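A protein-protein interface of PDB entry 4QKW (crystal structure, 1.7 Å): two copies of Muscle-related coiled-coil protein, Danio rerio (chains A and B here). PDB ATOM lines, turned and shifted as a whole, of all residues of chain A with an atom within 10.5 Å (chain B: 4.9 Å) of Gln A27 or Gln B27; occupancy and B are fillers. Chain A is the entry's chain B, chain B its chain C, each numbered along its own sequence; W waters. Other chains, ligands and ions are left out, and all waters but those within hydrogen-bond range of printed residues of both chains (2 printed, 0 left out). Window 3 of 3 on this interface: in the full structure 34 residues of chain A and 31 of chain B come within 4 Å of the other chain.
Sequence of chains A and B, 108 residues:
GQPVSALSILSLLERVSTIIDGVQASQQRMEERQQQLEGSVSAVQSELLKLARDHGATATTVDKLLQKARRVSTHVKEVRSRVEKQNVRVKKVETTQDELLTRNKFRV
OE2 of Glu B31 lies within hydrogen-bond range of OG of Ser A26, at 2.5 Å. The side-chain amide nitrogen of Gln B27 lies within hydrogen-bond range of the side-chain hydroxyl of Ser A26. SD of Met A30 sits close to NE2 of Gln B27 (3.6 Å).
The side-chain carboxylate (OE1) of Glu B31 sits at hydrogen-bond distance from the side-chain amide nitrogen (NE2) of Gln B28 (2.7 Å).
Among the printed residues, pairs that only touch across the chains: Ile A19 with Gln B24 (3.7 Å), Gln A27 with Gln B27 (3.7 Å), Met A30 with Met B30 (3.5 Å) and Met A30 with Glu B31 (3.3 Å).
Of the printed residues of chain B, Ile A19 touches Gln B24 (3.7 Å). Of the printed residues of chain B, Ser A26 touches Gln B27 and Glu B31. Gln A27 touches just one residue of chain B: Gln B27. Printed residues of chain B within 4 Å of Met A30: Gln B27, Met B30 and Glu B31. Of the printed residues of chain A, Gln B24 touches Ile A19. No residue of chain A comes within 4 Å of Ser B26. Of chain A, only Ser A26 (2.8 Å), Gln A27 (3.7 Å) and Met A30 (3.4 Å) come within 4 Å of Gln B27. Met B30 touches one residue of chain A. Glu B31 touches two residues of chain A. The nearest residue of chain A that does not touch Gln B27 is Val A23 (4.2 Å). The nearest printed residue of chain B that does not touch Ile A19 is Val B23 (6.4 Å).
Of the 17 printed residues of chain A, 4 touch a printed residue of chain B. Printed residues of chain A that touch a printed residue of chain B: Ile A19, Ser A26, Gln A27 and Met A30. Hydrophobic or aromatic side chains of chain A that line the printed part of chain B: Ile A19 and Met A30. Of the 9 printed residues of chain B, 4 touch a printed residue of chain A.
Ser A26 touches Glu B31, but with the chains exchanged Glu A31 does not touch Ser B26 (12.3 Å). Gln B27 touches its own counterpart, Gln A27. Met A30 touches Gln B27, but with the chains exchanged Gln A27 does not touch Met B30 (6.4 Å). Met A30 touches its own counterpart, Met B30. 9 positions are printed for both chains. Of the 7 pairs that touch across the chains among the printed residues, 2 have their exchanged pair printed and touching as well.
Water W1 bridges NH1 of Arg A33 (2.7 Å) and O of Glu B31 (2.8 Å). Water W2 lies within hydrogen-bond range of the backbone carbonyl oxygen of Ile A19 (3.1 Å) and the side-chain amide oxygen of Gln B24 (3.3 Å).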
ATOM      1  N   ILE A  19      22.253  25.049  -3.973  1.00  0.00           N
ATOM      2  CA  ILE A  19      22.220  23.982  -4.966  1.00  0.00           C
ATOM      3  C   ILE A  19      22.870  24.460  -6.269  1.00  0.00           C
ATOM      4  O   ILE A  19      23.654  23.722  -6.903  1.00  0.00           O
ATOM      5  CB  ILE A  19      20.768  23.494  -5.226  1.00  0.00           C
ATOM      6  CG1 ILE A  19      20.219  22.806  -3.975  1.00  0.00           C
ATOM      7  CG2 ILE A  19      20.754  22.490  -6.406  1.00  0.00           C
ATOM      8  CD1 ILE A  19      18.690  22.773  -3.908  1.00  0.00           C
ATOM      9  N   ILE A  20      22.576  25.695  -6.666  1.00  0.00           N
ATOM     10  CA  ILE A  20      23.202  26.269  -7.863  1.00  0.00           C
ATOM     11  C   ILE A  20      24.727  26.320  -7.718  1.00  0.00           C
ATOM     12  O   ILE A  20      25.451  25.954  -8.656  1.00  0.00           O
ATOM     13  CB  ILE A  20      22.647  27.664  -8.190  1.00  0.00           C
ATOM     14  CG1 ILE A  20      21.212  27.538  -8.696  1.00  0.00           C
ATOM     15  CG2 ILE A  20      23.509  28.366  -9.250  1.00  0.00           C
ATOM     16  CD1 ILE A  20      20.413  28.869  -8.734  1.00  0.00           C
ATOM     17  N   ASP A  21      25.218  26.754  -6.556  1.00  0.00           N
ATOM     18  CA  ASP A  21      26.665  26.760  -6.301  1.00  0.00           C
ATOM     19  C   ASP A  21      27.271  25.384  -6.509  1.00  0.00           C
ATOM     20  O   ASP A  21      28.323  25.251  -7.157  1.00  0.00           O
ATOM     21  CB  ASP A  21      26.986  27.255  -4.881  1.00  0.00           C
ATOM     22  CG  ASP A  21      26.722  28.727  -4.704  1.00  0.00           C
ATOM     23  OD1 ASP A  21      26.621  29.439  -5.720  1.00  0.00           O
ATOM     24  OD2 ASP A  21      26.613  29.167  -3.537  1.00  0.00           O
ATOM     25  N   GLY A  22      26.609  24.360  -5.971  1.00  0.00           N
ATOM     26  CA  GLY A  22      27.108  22.999  -6.090  1.00  0.00           C
ATOM     27  C   GLY A  22      27.099  22.500  -7.523  1.00  0.00           C
ATOM     28  O   GLY A  22      28.039  21.793  -7.948  1.00  0.00           O
ATOM     29  N   VAL A  23      26.042  22.827  -8.265  1.00  0.00           N
ATOM     30  CA  VAL A  23      25.972  22.435  -9.672  1.00  0.00           C
ATOM     31  C   VAL A  23      27.061  23.133 -10.471  1.00  0.00           C
ATOM     32  O   VAL A  23      27.743  22.502 -11.303  1.00  0.00           O
ATOM     33  CB  VAL A  23      24.589  22.702 -10.275  1.00  0.00           C
ATOM     34  CG1 VAL A  23      24.624  22.583 -11.808  1.00  0.00           C
ATOM     35  CG2 VAL A  23      23.575  21.716  -9.700  1.00  0.00           C
ATOM     36  N   GLN A  24      27.278  24.411 -10.186  1.00  0.00           N
ATOM     37  CA  GLN A  24      28.268  25.185 -10.939  1.00  0.00           C
ATOM     38  C   GLN A  24      29.694  24.714 -10.671  1.00  0.00           C
ATOM     39  O   GLN A  24      30.512  24.664 -11.591  1.00  0.00           O
ATOM     40  CB  GLN A  24      28.121  26.684 -10.655  1.00  0.00           C
ATOM     41  CG  GLN A  24      26.887  27.268 -11.342  1.00  0.00           C
ATOM     42  CD  GLN A  24      26.813  28.771 -11.252  1.00  0.00           C
ATOM     43  OE1 GLN A  24      26.975  29.355 -10.173  1.00  0.00           O
ATOM     44  NE2 GLN A  24      26.565  29.414 -12.387  1.00  0.00           N
ATOM     45  N   ALA A  25      29.990  24.381  -9.417  1.00  0.00           N
ATOM     46  CA  ALA A  25      31.282  23.761  -9.085  1.00  0.00           C
ATOM     47  C   ALA A  25      31.474  22.459  -9.861  1.00  0.00           C
ATOM     48  O   ALA A  25      32.548  22.201 -10.432  1.00  0.00           O
ATOM     49  CB  ALA A  25      31.375  23.504  -7.577  1.00  0.00           C
ATOM     50  N   SER A  26      30.440  21.624  -9.869  1.00  0.00           N
ATOM     51  CA  SER A  26      30.488  20.366 -10.604  1.00  0.00           C
ATOM     52  C   SER A  26      30.668  20.602 -12.096  1.00  0.00           C
ATOM     53  O   SER A  26      31.389  19.853 -12.756  1.00  0.00           O
ATOM     54  CB  SER A  26      29.218  19.548 -10.372  1.00  0.00           C
ATOM     55  OG  SER A  26      29.221  18.397 -11.206  1.00  0.00           O
ATOM     56  N   GLN A  27      30.013  21.628 -12.637  1.00  0.00           N
ATOM     57  CA  GLN A  27      30.149  21.921 -14.066  1.00  0.00           C
ATOM     58  C   GLN A  27      31.569  22.318 -14.450  1.00  0.00           C
ATOM     59  O   GLN A  27      32.043  21.971 -15.544  1.00  0.00           O
ATOM     60  CB  GLN A  27      29.163  22.999 -14.509  1.00  0.00           C
ATOM     61  CG  GLN A  27      27.751  22.488 -14.640  1.00  0.00           C
ATOM     62  CD  GLN A  27      26.795  23.554 -15.116  1.00  0.00           C
ATOM     63  OE1 GLN A  27      26.703  24.633 -14.526  1.00  0.00           O
ATOM     64  NE2 GLN A  27      26.091  23.267 -16.200  1.00  0.00           N
ATOM     65  N   GLN A  28      32.241  23.049 -13.563  1.00  0.00           N
ATOM     66  CA  GLN A  28      33.618  23.467 -13.806  1.00  0.00           C
ATOM     67  C   GLN A  28      34.538  22.261 -13.821  1.00  0.00           C
ATOM     68  O   GLN A  28      35.367  22.125 -14.722  1.00  0.00           O
ATOM     69  CB  GLN A  28      34.111  24.457 -12.746  1.00  0.00           C
ATOM     70  CG  GLN A  28      33.693  25.909 -12.962  1.00  0.00           C
ATOM     71  CD  GLN A  28      34.596  26.885 -12.221  1.00  0.00           C
ATOM     72  OE1 GLN A  28      35.235  26.529 -11.228  1.00  0.00           O
ATOM     73  NE2 GLN A  28      34.660  28.119 -12.708  1.00  0.00           N
ATOM     74  N   ARG A  29      34.407  21.396 -12.815  1.00  0.00           N
ATOM     75  CA  ARG A  29      35.213  20.171 -12.761  1.00  0.00           C
ATOM     76  C   ARG A  29      34.930  19.263 -13.961  1.00  0.00           C
ATOM     77  O   ARG A  29      35.840  18.624 -14.512  1.00  0.00           O
ATOM     78  CB  ARG A  29      34.975  19.402 -11.454  1.00  0.00           C
ATOM     79  CG  ARG A  29      35.350  20.177 -10.191  1.00  0.00           C
ATOM     80  CD  ARG A  29      35.171  19.325  -8.931  1.00  0.00           C
ATOM     81  NE  ARG A  29      33.771  19.002  -8.667  1.00  0.00           N
ATOM     82  CZ  ARG A  29      32.989  19.680  -7.828  1.00  0.00           C
ATOM     83  NH1 ARG A  29      33.470  20.716  -7.154  1.00  0.00           N
ATOM     84  NH2 ARG A  29      31.727  19.315  -7.652  1.00  0.00           N
ATOM     85  N   MET A  30      33.663  19.203 -14.354  1.00  0.00           N
ATOM     86  CA  MET A  30      33.226  18.403 -15.495  1.00  0.00           C
ATOM     87  C   MET A  30      33.845  18.922 -16.797  1.00  0.00           C
ATOM     88  O   MET A  30      34.274  18.140 -17.651  1.00  0.00           O
ATOM     89  CB  MET A  30      31.696  18.393 -15.562  1.00  0.00           C
ATOM     90  CG  MET A  30      31.094  17.533 -16.646  1.00  0.00           C
ATOM     91  SD  MET A  30      29.349  17.163 -16.342  1.00  0.00           S
ATOM     92  CE  MET A  30      29.510  16.158 -14.880  1.00  0.00           C
ATOM     93  N   GLU A  31      33.931  20.242 -16.935  1.00  0.00           N
ATOM     94  CA  GLU A  31      34.527  20.839 -18.129  1.00  0.00           C
ATOM     95  C   GLU A  31      36.026  20.545 -18.210  1.00  0.00           C
ATOM     96  O   GLU A  31      36.553  20.262 -19.289  1.00  0.00           O
ATOM     97  CB  GLU A  31      34.253  22.345 -18.162  1.00  0.00           C
ATOM     98  CG  GLU A  31      32.898  22.677 -18.782  1.00  0.00           C
ATOM     99  CD  GLU A  31      32.269  23.936 -18.224  1.00  0.00           C
ATOM    100  OE1 GLU A  31      33.009  24.800 -17.708  1.00  0.00           O
ATOM    101  OE2 GLU A  31      31.028  24.056 -18.301  1.00  0.00           O
ATOM    102  N   GLU A  32      36.707  20.614 -17.069  1.00  0.00           N
ATOM    103  CA  GLU A  32      38.132  20.287 -17.000  1.00  0.00           C
ATOM    104  C   GLU A  32      38.356  18.831 -17.376  1.00  0.00           C
ATOM    105  O   GLU A  32      39.233  18.524 -18.206  1.00  0.00           O
ATOM    106  CB  GLU A  32      38.675  20.579 -15.596  1.00  0.00           C
ATOM    107  CG  GLU A  32      38.489  22.033 -15.168  1.00  0.00           C
ATOM    108  CD  GLU A  32      38.693  22.254 -13.678  1.00  0.00           C
ATOM    109  OE1 GLU A  32      38.875  21.260 -12.936  1.00  0.00           O
ATOM    110  OE2 GLU A  32      38.666  23.428 -13.251  1.00  0.00           O
ATOM    111  N   ARG A  33      37.570  17.932 -16.784  1.00  0.00           N
ATOM    112  CA  ARG A  33      37.741  16.502 -17.056  1.00  0.00           C
ATOM    113  C   ARG A  33      37.353  16.161 -18.484  1.00  0.00           C
ATOM    114  O   ARG A  33      38.004  15.323 -19.128  1.00  0.00           O
ATOM    115  CB  ARG A  33      36.929  15.639 -16.084  1.00  0.00           C
ATOM    116  CG  ARG A  33      37.497  15.597 -14.669  1.00  0.00           C
ATOM    117  CD  ARG A  33      36.460  15.133 -13.636  1.00  0.00           C
ATOM    118  NE  ARG A  33      36.054  13.736 -13.807  1.00  0.00           N
ATOM    119  CZ  ARG A  33      34.788  13.328 -13.893  1.00  0.00           C
ATOM    120  NH1 ARG A  33      33.797  14.206 -13.832  1.00  0.00           N
ATOM    121  NH2 ARG A  33      34.507  12.041 -14.046  1.00  0.00           N
ATOM    122  N   GLN A  34      36.307  16.809 -18.992  1.00  0.00           N
ATOM    123  CA  GLN A  34      35.861  16.522 -20.356  1.00  0.00           C
ATOM    124  C   GLN A  34      36.941  16.847 -21.386  1.00  0.00           C
ATOM    125  O   GLN A  34      37.164  16.083 -22.338  1.00  0.00           O
ATOM    126  CB  GLN A  34      34.575  17.281 -20.690  1.00  0.00           C
ATOM    127  CG  GLN A  34      33.992  16.915 -22.063  1.00  0.00           C
ATOM    128  CD  GLN A  34      33.436  15.501 -22.118  1.00  0.00           C
ATOM    129  OE1 GLN A  34      33.164  14.888 -21.084  1.00  0.00           O
ATOM    130  NE2 GLN A  34      33.258  14.979 -23.327  1.00  0.00           N
ATOM    131  N   GLN A  35      37.632  17.966 -21.191  1.00  0.00           N
ATOM    132  CA  GLN A  35      38.691  18.364 -22.113  1.00  0.00           C
ATOM    133  C   GLN A  35      39.834  17.355 -22.075  1.00  0.00           C
ATOM    134  O   GLN A  35      40.407  17.007 -23.121  1.00  0.00           O
ATOM    135  CB  GLN A  35      39.201  19.771 -21.795  1.00  0.00           C
ATOM    136  CG  GLN A  35      40.395  20.200 -22.651  1.00  0.00           C
ATOM    137  CD  GLN A  35      40.713  21.678 -22.500  1.00  0.00           C
ATOM    138  OE1 GLN A  35      41.767  22.056 -21.991  1.00  0.00           O
ATOM    139  NE2 GLN A  35      39.799  22.514 -22.950  1.00  0.00           N
ATOM    140  N   VAL B  23      17.587  20.060 -12.488  1.00  0.00           N
ATOM    141  CA  VAL B  23      18.948  20.408 -12.915  1.00  0.00           C
ATOM    142  C   VAL B  23      19.986  19.674 -12.074  1.00  0.00           C
ATOM    143  O   VAL B  23      20.994  19.146 -12.598  1.00  0.00           O
ATOM    144  CB  VAL B  23      19.175  21.947 -12.836  1.00  0.00           C
ATOM    145  CG1 VAL B  23      20.657  22.297 -12.760  1.00  0.00           C
ATOM    146  CG2 VAL B  23      18.493  22.657 -14.011  1.00  0.00           C
ATOM    147  N   GLN B  24      19.752  19.638 -10.768  1.00  0.00           N
ATOM    148  CA  GLN B  24      20.648  18.938  -9.855  1.00  0.00           C
ATOM    149  C   GLN B  24      20.710  17.450 -10.194  1.00  0.00           C
ATOM    150  O   GLN B  24      21.799  16.868 -10.283  1.00  0.00           O
ATOM    151  CB  GLN B  24      20.189  19.135  -8.403  1.00  0.00           C
ATOM    152  CG  GLN B  24      21.088  18.438  -7.381  1.00  0.00           C
ATOM    153  CD  GLN B  24      20.749  18.821  -5.951  1.00  0.00           C
ATOM    154  OE1 GLN B  24      21.632  19.124  -5.149  1.00  0.00           O
ATOM    155  NE2 GLN B  24      19.466  18.802  -5.626  1.00  0.00           N
ATOM    156  N   ALA B  25      19.539  16.848 -10.396  1.00  0.00           N
ATOM    157  CA  ALA B  25      19.439  15.426 -10.728  1.00  0.00           C
ATOM    158  C   ALA B  25      20.135  15.143 -12.048  1.00  0.00           C
ATOM    159  O   ALA B  25      20.834  14.138 -12.188  1.00  0.00           O
ATOM    160  CB  ALA B  25      17.973  14.989 -10.794  1.00  0.00           C
ATOM    161  N   SER B  26      19.953  16.033 -13.020  1.00  0.00           N
ATOM    162  CA  SER B  26      20.647  15.897 -14.302  1.00  0.00           C
ATOM    163  C   SER B  26      22.166  15.993 -14.174  1.00  0.00           C
ATOM    164  O   SER B  26      22.899  15.243 -14.833  1.00  0.00           O
ATOM    165  CB  SER B  26      20.158  16.939 -15.311  1.00  0.00           C
ATOM    166  OG  SER B  26      18.828  16.671 -15.716  1.00  0.00           O
ATOM    167  N   GLN B  27      22.642  16.923 -13.348  1.00  0.00           N
ATOM    168  CA  GLN B  27      24.082  17.083 -13.151  1.00  0.00           C
ATOM    169  C   GLN B  27      24.686  15.827 -12.535  1.00  0.00           C
ATOM    170  O   GLN B  27      25.797  15.393 -12.898  1.00  0.00           O
ATOM    171  CB  GLN B  27      24.376  18.292 -12.255  1.00  0.00           C
ATOM    172  CG  GLN B  27      25.876  18.595 -12.139  1.00  0.00           C
ATOM    173  CD  GLN B  27      26.483  18.985 -13.472  1.00  0.00           C
ATOM    174  OE1 GLN B  27      25.767  19.401 -14.391  1.00  0.00           O
ATOM    175  NE2 GLN B  27      27.806  18.832 -13.597  1.00  0.00           N
ATOM    176  N   GLN B  28      23.952  15.233 -11.601  1.00  0.00           N
ATOM    177  CA  GLN B  28      24.396  13.984 -10.998  1.00  0.00           C
ATOM    178  C   GLN B  28      24.520  12.878 -12.044  1.00  0.00           C
ATOM    179  O   GLN B  28      25.491  12.111 -12.036  1.00  0.00           O
ATOM    180  CB  GLN B  28      23.462  13.564  -9.870  1.00  0.00           C
ATOM    181  CG  GLN B  28      23.763  14.287  -8.571  1.00  0.00           C
ATOM    182  CD  GLN B  28      25.248  14.292  -8.264  1.00  0.00           C
ATOM    183  OE1 GLN B  28      25.851  13.242  -8.034  1.00  0.00           O
ATOM    184  NE2 GLN B  28      25.853  15.478  -8.280  1.00  0.00           N
ATOM    185  N   ARG B  29      23.545  12.800 -12.948  1.00  0.00           N
ATOM    186  CA  ARG B  29      23.584  11.794 -14.015  1.00  0.00           C
ATOM    187  C   ARG B  29      24.754  12.010 -14.969  1.00  0.00           C
ATOM    188  O   ARG B  29      25.353  11.045 -15.469  1.00  0.00           O
ATOM    189  CB  ARG B  29      22.265  11.767 -14.793  1.00  0.00           C
ATOM    190  CG  ARG B  29      21.100  11.260 -13.957  1.00  0.00           C
ATOM    191  CD  ARG B  29      21.492   9.953 -13.293  1.00  0.00           C
ATOM    192  NE  ARG B  29      20.585   9.563 -12.219  1.00  0.00           N
ATOM    193  CZ  ARG B  29      20.879   9.644 -10.927  1.00  0.00           C
ATOM    194  NH1 ARG B  29      22.063  10.101 -10.542  1.00  0.00           N
ATOM    195  NH2 ARG B  29      19.992   9.264 -10.017  1.00  0.00           N
ATOM    196  N   MET B  30      25.069  13.268 -15.211  1.00  0.00           N
ATOM    197  CA  MET B  30      26.182  13.633 -16.070  1.00  0.00           C
ATOM    198  C   MET B  30      27.547  13.307 -15.443  1.00  0.00           C
ATOM    199  O   MET B  30      28.450  12.885 -16.133  1.00  0.00           O
ATOM    200  CB  MET B  30      26.096  15.076 -16.510  1.00  0.00           C
ATOM    201  CG  MET B  30      24.885  15.361 -17.370  1.00  0.00           C
ATOM    202  SD  MET B  30      24.558  17.078 -17.717  1.00  0.00           S
ATOM    203  CE  MET B  30      25.898  17.376 -18.802  1.00  0.00           C
ATOM    204  N   GLU B  31      27.649  13.505 -14.139  1.00  0.00           N
ATOM    205  CA  GLU B  31      28.802  13.127 -13.361  1.00  0.00           C
ATOM    206  C   GLU B  31      29.046  11.658 -13.460  1.00  0.00           C
ATOM    207  O   GLU B  31      30.139  11.216 -13.589  1.00  0.00           O
ATOM    208  CB  GLU B  31      28.615  13.497 -11.907  1.00  0.00           C
ATOM    209  CG  GLU B  31      28.823  14.949 -11.607  1.00  0.00           C
ATOM    210  CD  GLU B  31      28.572  15.292 -10.176  1.00  0.00           C
ATOM    211  OE1 GLU B  31      28.045  14.464  -9.441  1.00  0.00           O
ATOM    212  OE2 GLU B  31      28.902  16.401  -9.796  1.00  0.00           O
HETATM  213  O   HOH W   1      32.355  12.402 -12.354  1.00  0.00           O
HETATM  214  O   HOH W   2      24.357  20.985  -5.578  1.00  0.00           O
